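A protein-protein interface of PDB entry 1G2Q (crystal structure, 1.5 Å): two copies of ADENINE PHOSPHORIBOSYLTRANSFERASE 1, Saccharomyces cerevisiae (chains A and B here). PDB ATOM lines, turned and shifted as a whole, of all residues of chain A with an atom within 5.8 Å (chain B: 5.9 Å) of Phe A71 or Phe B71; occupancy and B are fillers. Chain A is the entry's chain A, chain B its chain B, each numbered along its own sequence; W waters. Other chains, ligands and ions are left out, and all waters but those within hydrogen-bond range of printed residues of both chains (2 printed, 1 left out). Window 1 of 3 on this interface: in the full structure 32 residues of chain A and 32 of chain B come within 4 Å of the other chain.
Hydrophobic or aromatic side chains of chain A within 4 Å of the printed part of chain B: Phe A71, Leu A72, Pro A75 and Phe A85.
Hydrophobic or aromatic side chains of chain B that line the printed part of chain A: Phe B71, Leu B72, Pro B75 and Phe B85.
Along chain B the printed residues that touch a printed residue of chain A span positions 67 to 89.
Among the printed residues, 17 pairs touch across the chains.
Among the printed residues, no Asp or Glu carboxylate lies within 4 Å of a Lys or Arg side-chain nitrogen of the other chain.
The backbone NH (N) of Glu B67 sits at hydrogen-bond distance from the backbone carbonyl oxygen (O) of Val B88 (3.1 Å).
OE2 of Glu A67 lies within salt-bridge range of NH2 of Arg A89, at 2.8 Å.
The guanidinium group (NE) of Arg B89 is in salt-bridge range of the side-chain carboxylate (OE1) of Glu B67 (2.8 Å).
The backbone NH of Glu A67 is in hydrogen-bond range of the backbone carbonyl oxygen of Val A88.
Of chain B, only Ser B68, Phe B71 and Leu B72 come within 4 Å of Phe A71.
Of the printed residues of chain A, Glu B67 touches Ser A68.
Phe B71 touches just these residues of chain A: Ser A68, Phe A71 and Leu A72.
Pro B87 touches none of the printed residues of chain A.
Of the printed residues of chain A, Arg B89 touches Ser A68 (2.9 Å) and Arg A69 (3.6 Å).
The nearest residue of chain B that does not touch Phe A71 is Pro B75 (4.7 Å).
The nearest residue of chain A that does not touch Phe B71 is Pro A75 (4.7 Å).
The nearest printed residue of chain A that does not touch Phe B85 is Phe A71 (7.3 Å).
The side-chain hydroxyl (OG1) of Thr A76 sits at hydrogen-bond distance from the side-chain hydroxyl (OG1) of Thr B76.
OG of Ser B68 is in hydrogen-bond range of OE2 of Glu A67.
O of Phe A71 sits close to O of Phe B71.
The side-chain hydroxyl (OG) of Ser A68 lies within hydrogen-bond range of the guanidinium group (NH2) of Arg B89 (2.9 Å).
Among the printed residues, merely in contact across the chains: Ser A68 with Glu B67, Ser A68 with Ser B68, Ser A68 with Phe B71, Arg A69 with Arg B89, Phe A71 with Ser B68, Phe A71 with Leu B72, Leu A72 with Phe B71, Leu A72 with Pro B75, Leu A72 with Phe B85, Pro A75 with Leu B72, Phe A85 with Leu B72, Arg A89 with Ser B68 and Arg A89 with Arg B69.
Water W2 lies within hydrogen-bond range of the guanidinium group of Arg A69 (3.1 Å) and the guanidinium group of Arg B89 (3.2 Å).
Water W1 lies within hydrogen-bond range of NE of Arg B69 (3.2 Å) and NH1 of Arg A89 (3.3 Å).
Glu A67 touches Ser B68, and with the chains exchanged Ser A68 touches Glu B67.
Arg A69 touches Arg B89, and with the chains exchanged Arg A89 touches Arg B69.
Phe A71 touches Leu B72, and with the chains exchanged Leu A72 touches Phe B71.
Thr A76 touches its own counterpart, Thr B76.
Of the 17 pairs that touch across the chains among the printed residues, 17 have their exchanged pair printed and touching as well.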
ATOM      1  N   GLY A  65      -6.532 -14.597   9.459  1.00  0.00           N
ATOM      2  CA  GLY A  65      -5.799 -15.632  10.168  1.00  0.00           C
ATOM      3  C   GLY A  65      -4.627 -15.123  10.978  1.00  0.00           C
ATOM      4  O   GLY A  65      -3.925 -14.212  10.544  1.00  0.00           O
ATOM      5  N   LEU A  66      -4.413 -15.708  12.155  1.00  0.00           N
ATOM      6  CA  LEU A  66      -3.311 -15.287  13.017  1.00  0.00           C
ATOM      7  C   LEU A  66      -2.014 -16.046  12.713  1.00  0.00           C
ATOM      8  O   LEU A  66      -2.035 -17.261  12.490  1.00  0.00           O
ATOM      9  CB  LEU A  66      -3.691 -15.485  14.490  1.00  0.00           C
ATOM     10  CG  LEU A  66      -5.042 -14.903  14.936  1.00  0.00           C
ATOM     11  CD1 LEU A  66      -5.126 -14.962  16.457  1.00  0.00           C
ATOM     12  CD2 LEU A  66      -5.205 -13.473  14.451  1.00  0.00           C
ATOM     13  N   GLU A  67      -0.895 -15.323  12.693  1.00  0.00           N
ATOM     14  CA  GLU A  67       0.407 -15.916  12.424  1.00  0.00           C
ATOM     15  C   GLU A  67       0.803 -16.847  13.569  1.00  0.00           C
ATOM     16  O   GLU A  67       0.716 -16.463  14.733  1.00  0.00           O
ATOM     17  CB  GLU A  67       1.460 -14.819  12.273  1.00  0.00           C
ATOM     18  CG  GLU A  67       2.778 -15.337  11.749  1.00  0.00           C
ATOM     19  CD  GLU A  67       3.849 -14.273  11.666  1.00  0.00           C
ATOM     20  OE1 GLU A  67       3.526 -13.071  11.760  1.00  0.00           O
ATOM     21  OE2 GLU A  67       5.025 -14.646  11.506  1.00  0.00           O
ATOM     22  N   SER A  68       1.233 -18.064  13.246  1.00  0.00           N
ATOM     23  CA  SER A  68       1.325 -18.523  11.869  1.00  0.00           C
ATOM     24  C   SER A  68       0.509 -19.807  11.686  1.00  0.00           C
ATOM     25  O   SER A  68       0.291 -20.264  10.567  1.00  0.00           O
ATOM     26  CB  SER A  68       2.794 -18.751  11.487  1.00  0.00           C
ATOM     27  OG  SER A  68       3.341 -19.835  12.204  1.00  0.00           O
ATOM     28  N   ARG A  69       0.013 -20.377  12.785  1.00  0.00           N
ATOM     29  CA  ARG A  69      -0.795 -21.591  12.677  1.00  0.00           C
ATOM     30  C   ARG A  69      -2.132 -21.311  11.995  1.00  0.00           C
ATOM     31  O   ARG A  69      -2.699 -22.187  11.339  1.00  0.00           O
ATOM     32  CB  ARG A  69      -0.995 -22.227  14.057  1.00  0.00           C
ATOM     33  CG  ARG A  69       0.283 -22.873  14.570  1.00  0.00           C
ATOM     34  CD  ARG A  69       0.190 -23.340  16.018  1.00  0.00           C
ATOM     35  NE  ARG A  69       1.432 -23.988  16.438  1.00  0.00           N
ATOM     36  CZ  ARG A  69       1.960 -23.905  17.656  1.00  0.00           C
ATOM     37  NH1 ARG A  69       1.362 -23.196  18.601  1.00  0.00           N
ATOM     38  NH2 ARG A  69       3.095 -24.538  17.930  1.00  0.00           N
ATOM     39  N   GLY A  70      -2.625 -20.082  12.132  1.00  0.00           N
ATOM     40  CA  GLY A  70      -3.864 -19.712  11.474  1.00  0.00           C
ATOM     41  C   GLY A  70      -3.657 -19.624   9.966  1.00  0.00           C
ATOM     42  O   GLY A  70      -4.614 -19.658   9.192  1.00  0.00           O
ATOM     43  N   PHE A  71      -2.398 -19.490   9.551  1.00  0.00           N
ATOM     44  CA  PHE A  71      -2.053 -19.413   8.132  1.00  0.00           C
ATOM     45  C   PHE A  71      -2.146 -20.785   7.485  1.00  0.00           C
ATOM     46  O   PHE A  71      -2.252 -20.891   6.268  1.00  0.00           O
ATOM     47  CB  PHE A  71      -0.607 -18.937   7.924  1.00  0.00           C
ATOM     48  CG  PHE A  71      -0.356 -17.497   8.272  1.00  0.00           C
ATOM     49  CD1 PHE A  71      -1.351 -16.688   8.813  1.00  0.00           C
ATOM     50  CD2 PHE A  71       0.909 -16.953   8.062  1.00  0.00           C
ATOM     51  CE1 PHE A  71      -1.079 -15.356   9.137  1.00  0.00           C
ATOM     52  CE2 PHE A  71       1.187 -15.631   8.382  1.00  0.00           C
ATOM     53  CZ  PHE A  71       0.190 -14.830   8.922  1.00  0.00           C
ATOM     54  N   LEU A  72      -2.081 -21.836   8.299  1.00  0.00           N
ATOM     55  CA  LEU A  72      -2.121 -23.188   7.772  1.00  0.00           C
ATOM     56  C   LEU A  72      -3.472 -23.605   7.199  1.00  0.00           C
ATOM     57  O   LEU A  72      -3.524 -24.339   6.216  1.00  0.00           O
ATOM     58  CB  LEU A  72      -1.652 -24.178   8.850  1.00  0.00           C
ATOM     59  CG  LEU A  72      -0.151 -24.057   9.162  1.00  0.00           C
ATOM     60  CD1 LEU A  72       0.219 -24.877  10.383  1.00  0.00           C
ATOM     61  CD2 LEU A  72       0.649 -24.524   7.952  1.00  0.00           C
ATOM     62  N   PHE A  73      -4.566 -23.127   7.787  1.00  0.00           N
ATOM     63  CA  PHE A  73      -5.886 -23.496   7.278  1.00  0.00           C
ATOM     64  C   PHE A  73      -6.778 -22.307   6.926  1.00  0.00           C
ATOM     65  O   PHE A  73      -7.754 -22.460   6.189  1.00  0.00           O
ATOM     66  CB  PHE A  73      -6.623 -24.408   8.276  1.00  0.00           C
ATOM     67  CG  PHE A  73      -7.080 -23.708   9.532  1.00  0.00           C
ATOM     68  CD1 PHE A  73      -6.206 -23.503  10.594  1.00  0.00           C
ATOM     69  CD2 PHE A  73      -8.395 -23.260   9.650  1.00  0.00           C
ATOM     70  CE1 PHE A  73      -6.635 -22.860  11.765  1.00  0.00           C
ATOM     71  CE2 PHE A  73      -8.834 -22.614  10.817  1.00  0.00           C
ATOM     72  CZ  PHE A  73      -7.952 -22.415  11.875  1.00  0.00           C
ATOM     73  N   GLY A  74      -6.445 -21.126   7.445  1.00  0.00           N
ATOM     74  CA  GLY A  74      -7.247 -19.943   7.171  1.00  0.00           C
ATOM     75  C   GLY A  74      -7.377 -19.609   5.694  1.00  0.00           C
ATOM     76  O   GLY A  74      -8.488 -19.395   5.193  1.00  0.00           O
ATOM     77  N   PRO A  75      -6.254 -19.521   4.965  1.00  0.00           N
ATOM     78  CA  PRO A  75      -6.331 -19.207   3.534  1.00  0.00           C
ATOM     79  C   PRO A  75      -7.130 -20.267   2.778  1.00  0.00           C
ATOM     80  O   PRO A  75      -7.942 -19.941   1.918  1.00  0.00           O
ATOM     81  CB  PRO A  75      -4.863 -19.177   3.107  1.00  0.00           C
ATOM     82  CG  PRO A  75      -4.162 -18.736   4.367  1.00  0.00           C
ATOM     83  CD  PRO A  75      -4.854 -19.557   5.422  1.00  0.00           C
ATOM     84  N   THR A  76      -6.895 -21.536   3.114  1.00  0.00           N
ATOM     85  CA  THR A  76      -7.591 -22.646   2.470  1.00  0.00           C
ATOM     86  C   THR A  76      -9.101 -22.520   2.685  1.00  0.00           C
ATOM     87  O   THR A  76      -9.887 -22.667   1.747  1.00  0.00           O
ATOM     88  CB  THR A  76      -7.098 -23.985   3.032  1.00  0.00           C
ATOM     89  OG1 THR A  76      -5.665 -24.032   2.938  1.00  0.00           O
ATOM     90  CG2 THR A  76      -7.686 -25.144   2.238  1.00  0.00           C
ATOM     91  N   PHE A  85      -8.735 -13.523   2.121  1.00  0.00           N
ATOM     92  CA  PHE A  85      -7.955 -13.857   3.305  1.00  0.00           C
ATOM     93  C   PHE A  85      -6.964 -12.738   3.590  1.00  0.00           C
ATOM     94  O   PHE A  85      -6.303 -12.236   2.678  1.00  0.00           O
ATOM     95  CB  PHE A  85      -7.151 -15.149   3.128  1.00  0.00           C
ATOM     96  CG  PHE A  85      -6.232 -15.432   4.286  1.00  0.00           C
ATOM     97  CD1 PHE A  85      -6.712 -16.065   5.433  1.00  0.00           C
ATOM     98  CD2 PHE A  85      -4.913 -14.965   4.279  1.00  0.00           C
ATOM     99  CE1 PHE A  85      -5.897 -16.222   6.562  1.00  0.00           C
ATOM    100  CE2 PHE A  85      -4.091 -15.116   5.402  1.00  0.00           C
ATOM    101  CZ  PHE A  85      -4.584 -15.742   6.541  1.00  0.00           C
ATOM    102  N   PRO A  87      -3.893 -11.662   6.598  1.00  0.00           N
ATOM    103  CA  PRO A  87      -3.156 -12.104   7.779  1.00  0.00           C
ATOM    104  C   PRO A  87      -2.924 -11.026   8.829  1.00  0.00           C
ATOM    105  O   PRO A  87      -2.831  -9.842   8.512  1.00  0.00           O
ATOM    106  CB  PRO A  87      -1.827 -12.557   7.183  1.00  0.00           C
ATOM    107  CG  PRO A  87      -1.587 -11.469   6.143  1.00  0.00           C
ATOM    108  CD  PRO A  87      -2.972 -11.297   5.502  1.00  0.00           C
ATOM    109  N   VAL A  88      -2.847 -11.456  10.081  1.00  0.00           N
ATOM    110  CA  VAL A  88      -2.478 -10.571  11.179  1.00  0.00           C
ATOM    111  C   VAL A  88      -1.089 -11.135  11.466  1.00  0.00           C
ATOM    112  O   VAL A  88      -0.924 -12.356  11.579  1.00  0.00           O
ATOM    113  CB  VAL A  88      -3.371 -10.740  12.431  1.00  0.00           C
ATOM    114  CG1 VAL A  88      -2.663 -10.150  13.654  1.00  0.00           C
ATOM    115  CG2 VAL A  88      -4.699 -10.023  12.213  1.00  0.00           C
ATOM    116  N   ARG A  89      -0.087 -10.273  11.543  1.00  0.00           N
ATOM    117  CA  ARG A  89       1.265 -10.749  11.800  1.00  0.00           C
ATOM    118  C   ARG A  89       1.886 -10.109  13.014  1.00  0.00           C
ATOM    119  O   ARG A  89       1.406  -9.096  13.515  1.00  0.00           O
ATOM    120  CB  ARG A  89       2.185 -10.470  10.607  1.00  0.00           C
ATOM    121  CG  ARG A  89       1.749 -11.091   9.290  1.00  0.00           C
ATOM    122  CD  ARG A  89       2.951 -11.314   8.375  1.00  0.00           C
ATOM    123  NE  ARG A  89       3.881 -12.267   8.971  1.00  0.00           N
ATOM    124  CZ  ARG A  89       5.017 -12.664   8.405  1.00  0.00           C
ATOM    125  NH1 ARG A  89       5.371 -12.189   7.217  1.00  0.00           N
ATOM    126  NH2 ARG A  89       5.796 -13.536   9.031  1.00  0.00           N
ATOM    127  N   GLY B  65       6.127 -26.324   2.972  1.00  0.00           N
ATOM    128  CA  GLY B  65       6.074 -24.869   2.976  1.00  0.00           C
ATOM    129  C   GLY B  65       6.923 -24.229   4.055  1.00  0.00           C
ATOM    130  O   GLY B  65       6.979 -24.718   5.182  1.00  0.00           O
ATOM    131  N   LEU B  66       7.594 -23.129   3.716  1.00  0.00           N
ATOM    132  CA  LEU B  66       8.454 -22.452   4.686  1.00  0.00           C
ATOM    133  C   LEU B  66       7.695 -21.390   5.487  1.00  0.00           C
ATOM    134  O   LEU B  66       6.896 -20.648   4.922  1.00  0.00           O
ATOM    135  CB  LEU B  66       9.647 -21.814   3.963  1.00  0.00           C
ATOM    136  CG  LEU B  66      10.362 -22.708   2.937  1.00  0.00           C
ATOM    137  CD1 LEU B  66      11.636 -22.020   2.456  1.00  0.00           C
ATOM    138  CD2 LEU B  66      10.691 -24.057   3.562  1.00  0.00           C
ATOM    139  N   GLU B  67       7.946 -21.313   6.795  1.00  0.00           N
ATOM    140  CA  GLU B  67       7.268 -20.336   7.635  1.00  0.00           C
ATOM    141  C   GLU B  67       7.764 -18.942   7.225  1.00  0.00           C
ATOM    142  O   GLU B  67       8.966 -18.751   7.038  1.00  0.00           O
ATOM    143  CB  GLU B  67       7.613 -20.621   9.103  1.00  0.00           C
ATOM    144  CG  GLU B  67       6.837 -19.792  10.113  1.00  0.00           C
ATOM    145  CD  GLU B  67       7.205 -20.099  11.558  1.00  0.00           C
ATOM    146  OE1 GLU B  67       7.878 -21.115  11.823  1.00  0.00           O
ATOM    147  OE2 GLU B  67       6.823 -19.308  12.440  1.00  0.00           O
ATOM    148  N   SER B  68       6.868 -17.964   7.082  1.00  0.00           N
ATOM    149  CA  SER B  68       5.432 -18.114   7.288  1.00  0.00           C
ATOM    150  C   SER B  68       4.668 -17.908   5.977  1.00  0.00           C
ATOM    151  O   SER B  68       3.525 -18.331   5.848  1.00  0.00           O
ATOM    152  CB  SER B  68       4.932 -17.079   8.299  1.00  0.00           C
ATOM    153  OG  SER B  68       5.350 -17.385   9.616  1.00  0.00           O
ATOM    154  N   ARG B  69       5.320 -17.247   5.023  1.00  0.00           N
ATOM    155  CA  ARG B  69       4.698 -16.944   3.744  1.00  0.00           C
ATOM    156  C   ARG B  69       4.383 -18.173   2.902  1.00  0.00           C
ATOM    157  O   ARG B  69       3.422 -18.167   2.135  1.00  0.00           O
ATOM    158  CB  ARG B  69       5.576 -15.947   2.974  1.00  0.00           C
ATOM    159  CG  ARG B  69       5.644 -14.601   3.691  1.00  0.00           C
ATOM    160  CD  ARG B  69       6.532 -13.579   2.998  1.00  0.00           C
ATOM    161  NE  ARG B  69       6.445 -12.267   3.648  1.00  0.00           N
ATOM    162  CZ  ARG B  69       7.487 -11.478   3.897  1.00  0.00           C
ATOM    163  NH1 ARG B  69       8.711 -11.861   3.556  1.00  0.00           N
ATOM    164  NH2 ARG B  69       7.307 -10.305   4.490  1.00  0.00           N
ATOM    165  N   GLY B  70       5.183 -19.227   3.048  1.00  0.00           N
ATOM    166  CA  GLY B  70       4.918 -20.451   2.312  1.00  0.00           C
ATOM    167  C   GLY B  70       3.655 -21.114   2.840  1.00  0.00           C
ATOM    168  O   GLY B  70       3.048 -21.947   2.168  1.00  0.00           O
ATOM    169  N   PHE B  71       3.255 -20.750   4.059  1.00  0.00           N
ATOM    170  CA  PHE B  71       2.046 -21.306   4.672  1.00  0.00           C
ATOM    171  C   PHE B  71       0.802 -20.701   4.026  1.00  0.00           C
ATOM    172  O   PHE B  71      -0.276 -21.298   4.059  1.00  0.00           O
ATOM    173  CB  PHE B  71       1.973 -20.971   6.175  1.00  0.00           C
ATOM    174  CG  PHE B  71       3.007 -21.654   7.041  1.00  0.00           C
ATOM    175  CD1 PHE B  71       3.985 -22.493   6.506  1.00  0.00           C
ATOM    176  CD2 PHE B  71       2.986 -21.446   8.420  1.00  0.00           C
ATOM    177  CE1 PHE B  71       4.922 -23.108   7.340  1.00  0.00           C
ATOM    178  CE2 PHE B  71       3.914 -22.052   9.254  1.00  0.00           C
ATOM    179  CZ  PHE B  71       4.884 -22.885   8.714  1.00  0.00           C
ATOM    180  N   LEU B  72       0.940 -19.509   3.454  1.00  0.00           N
ATOM    181  CA  LEU B  72      -0.201 -18.838   2.853  1.00  0.00           C
ATOM    182  C   LEU B  72      -0.777 -19.530   1.617  1.00  0.00           C
ATOM    183  O   LEU B  72      -2.000 -19.493   1.399  1.00  0.00           O
ATOM    184  CB  LEU B  72       0.148 -17.371   2.554  1.00  0.00           C
ATOM    185  CG  LEU B  72       0.419 -16.528   3.811  1.00  0.00           C
ATOM    186  CD1 LEU B  72       0.921 -15.146   3.428  1.00  0.00           C
ATOM    187  CD2 LEU B  72      -0.851 -16.426   4.649  1.00  0.00           C
ATOM    188  N   PHE B  73       0.075 -20.183   0.827  1.00  0.00           N
ATOM    189  CA  PHE B  73      -0.404 -20.875  -0.374  1.00  0.00           C
ATOM    190  C   PHE B  73      -0.039 -22.356  -0.465  1.00  0.00           C
ATOM    191  O   PHE B  73      -0.678 -23.108  -1.205  1.00  0.00           O
ATOM    192  CB  PHE B  73       0.071 -20.152  -1.651  1.00  0.00           C
ATOM    193  CG  PHE B  73       1.551 -20.269  -1.924  1.00  0.00           C
ATOM    194  CD1 PHE B  73       2.467 -19.443  -1.277  1.00  0.00           C
ATOM    195  CD2 PHE B  73       2.023 -21.184  -2.865  1.00  0.00           C
ATOM    196  CE1 PHE B  73       3.840 -19.524  -1.565  1.00  0.00           C
ATOM    197  CE2 PHE B  73       3.386 -21.279  -3.163  1.00  0.00           C
ATOM    198  CZ  PHE B  73       4.299 -20.448  -2.516  1.00  0.00           C
ATOM    199  N   GLY B  74       0.978 -22.770   0.288  1.00  0.00           N
ATOM    200  CA  GLY B  74       1.406 -24.160   0.252  1.00  0.00           C
ATOM    201  C   GLY B  74       0.351 -25.192   0.618  1.00  0.00           C
ATOM    202  O   GLY B  74       0.164 -26.175  -0.106  1.00  0.00           O
ATOM    203  N   PRO B  75      -0.352 -25.012   1.741  1.00  0.00           N
ATOM    204  CA  PRO B  75      -1.376 -25.983   2.132  1.00  0.00           C
ATOM    205  C   PRO B  75      -2.494 -26.118   1.097  1.00  0.00           C
ATOM    206  O   PRO B  75      -2.961 -27.224   0.826  1.00  0.00           O
ATOM    207  CB  PRO B  75      -1.881 -25.433   3.468  1.00  0.00           C
ATOM    208  CG  PRO B  75      -0.668 -24.714   4.017  1.00  0.00           C
ATOM    209  CD  PRO B  75      -0.146 -24.006   2.797  1.00  0.00           C
ATOM    210  N   THR B  76      -2.925 -24.995   0.529  1.00  0.00           N
ATOM    211  CA  THR B  76      -3.991 -25.018  -0.466  1.00  0.00           C
ATOM    212  C   THR B  76      -3.504 -25.706  -1.740  1.00  0.00           C
ATOM    213  O   THR B  76      -4.246 -26.458  -2.370  1.00  0.00           O
ATOM    214  CB  THR B  76      -4.483 -23.593  -0.782  1.00  0.00           C
ATOM    215  OG1 THR B  76      -4.982 -22.984   0.419  1.00  0.00           O
ATOM    216  CG2 THR B  76      -5.596 -23.633  -1.815  1.00  0.00           C
ATOM    217  N   PHE B  85       0.691 -31.825   3.194  1.00  0.00           N
ATOM    218  CA  PHE B  85       1.439 -30.596   3.442  1.00  0.00           C
ATOM    219  C   PHE B  85       2.199 -30.724   4.758  1.00  0.00           C
ATOM    220  O   PHE B  85       1.651 -31.185   5.753  1.00  0.00           O
ATOM    221  CB  PHE B  85       0.521 -29.378   3.557  1.00  0.00           C
ATOM    222  CG  PHE B  85       1.261 -28.123   3.933  1.00  0.00           C
ATOM    223  CD1 PHE B  85       1.898 -27.363   2.958  1.00  0.00           C
ATOM    224  CD2 PHE B  85       1.399 -27.752   5.272  1.00  0.00           C
ATOM    225  CE1 PHE B  85       2.670 -26.253   3.301  1.00  0.00           C
ATOM    226  CE2 PHE B  85       2.170 -26.642   5.630  1.00  0.00           C
ATOM    227  CZ  PHE B  85       2.807 -25.892   4.648  1.00  0.00           C
ATOM    228  N   PRO B  87       5.078 -28.406   7.237  1.00  0.00           N
ATOM    229  CA  PRO B  87       5.792 -27.141   7.399  1.00  0.00           C
ATOM    230  C   PRO B  87       7.222 -27.267   7.884  1.00  0.00           C
ATOM    231  O   PRO B  87       7.585 -28.233   8.558  1.00  0.00           O
ATOM    232  CB  PRO B  87       4.957 -26.419   8.444  1.00  0.00           C
ATOM    233  CG  PRO B  87       4.588 -27.558   9.375  1.00  0.00           C
ATOM    234  CD  PRO B  87       4.215 -28.676   8.405  1.00  0.00           C
ATOM    235  N   VAL B  88       8.022 -26.270   7.527  1.00  0.00           N
ATOM    236  CA  VAL B  88       9.381 -26.147   8.030  1.00  0.00           C
ATOM    237  C   VAL B  88       9.193 -24.891   8.876  1.00  0.00           C
ATOM    238  O   VAL B  88       8.660 -23.887   8.394  1.00  0.00           O
ATOM    239  CB  VAL B  88      10.428 -25.866   6.928  1.00  0.00           C
ATOM    240  CG1 VAL B  88      11.703 -25.312   7.558  1.00  0.00           C
ATOM    241  CG2 VAL B  88      10.745 -27.159   6.180  1.00  0.00           C
ATOM    242  N   ARG B  89       9.592 -24.955  10.138  1.00  0.00           N
ATOM    243  CA  ARG B  89       9.432 -23.803  11.021  1.00  0.00           C
ATOM    244  C   ARG B  89      10.748 -23.351  11.623  1.00  0.00           C
ATOM    245  O   ARG B  89      11.743 -24.073  11.582  1.00  0.00           O
ATOM    246  CB  ARG B  89       8.478 -24.140  12.176  1.00  0.00           C
ATOM    247  CG  ARG B  89       7.060 -24.511  11.762  1.00  0.00           C
ATOM    248  CD  ARG B  89       6.064 -24.194  12.881  1.00  0.00           C
ATOM    249  NE  ARG B  89       5.998 -22.752  13.130  1.00  0.00           N
ATOM    250  CZ  ARG B  89       5.198 -22.176  14.025  1.00  0.00           C
ATOM    251  NH1 ARG B  89       4.382 -22.914  14.767  1.00  0.00           N
ATOM    252  NH2 ARG B  89       5.218 -20.857  14.180  1.00  0.00           N
HETATM  253  O   HOH W   1       3.986 -10.592   4.686  1.00  0.00           O
HETATM  254  O   HOH W   2       3.361 -25.955  14.996  1.00  0.00           O
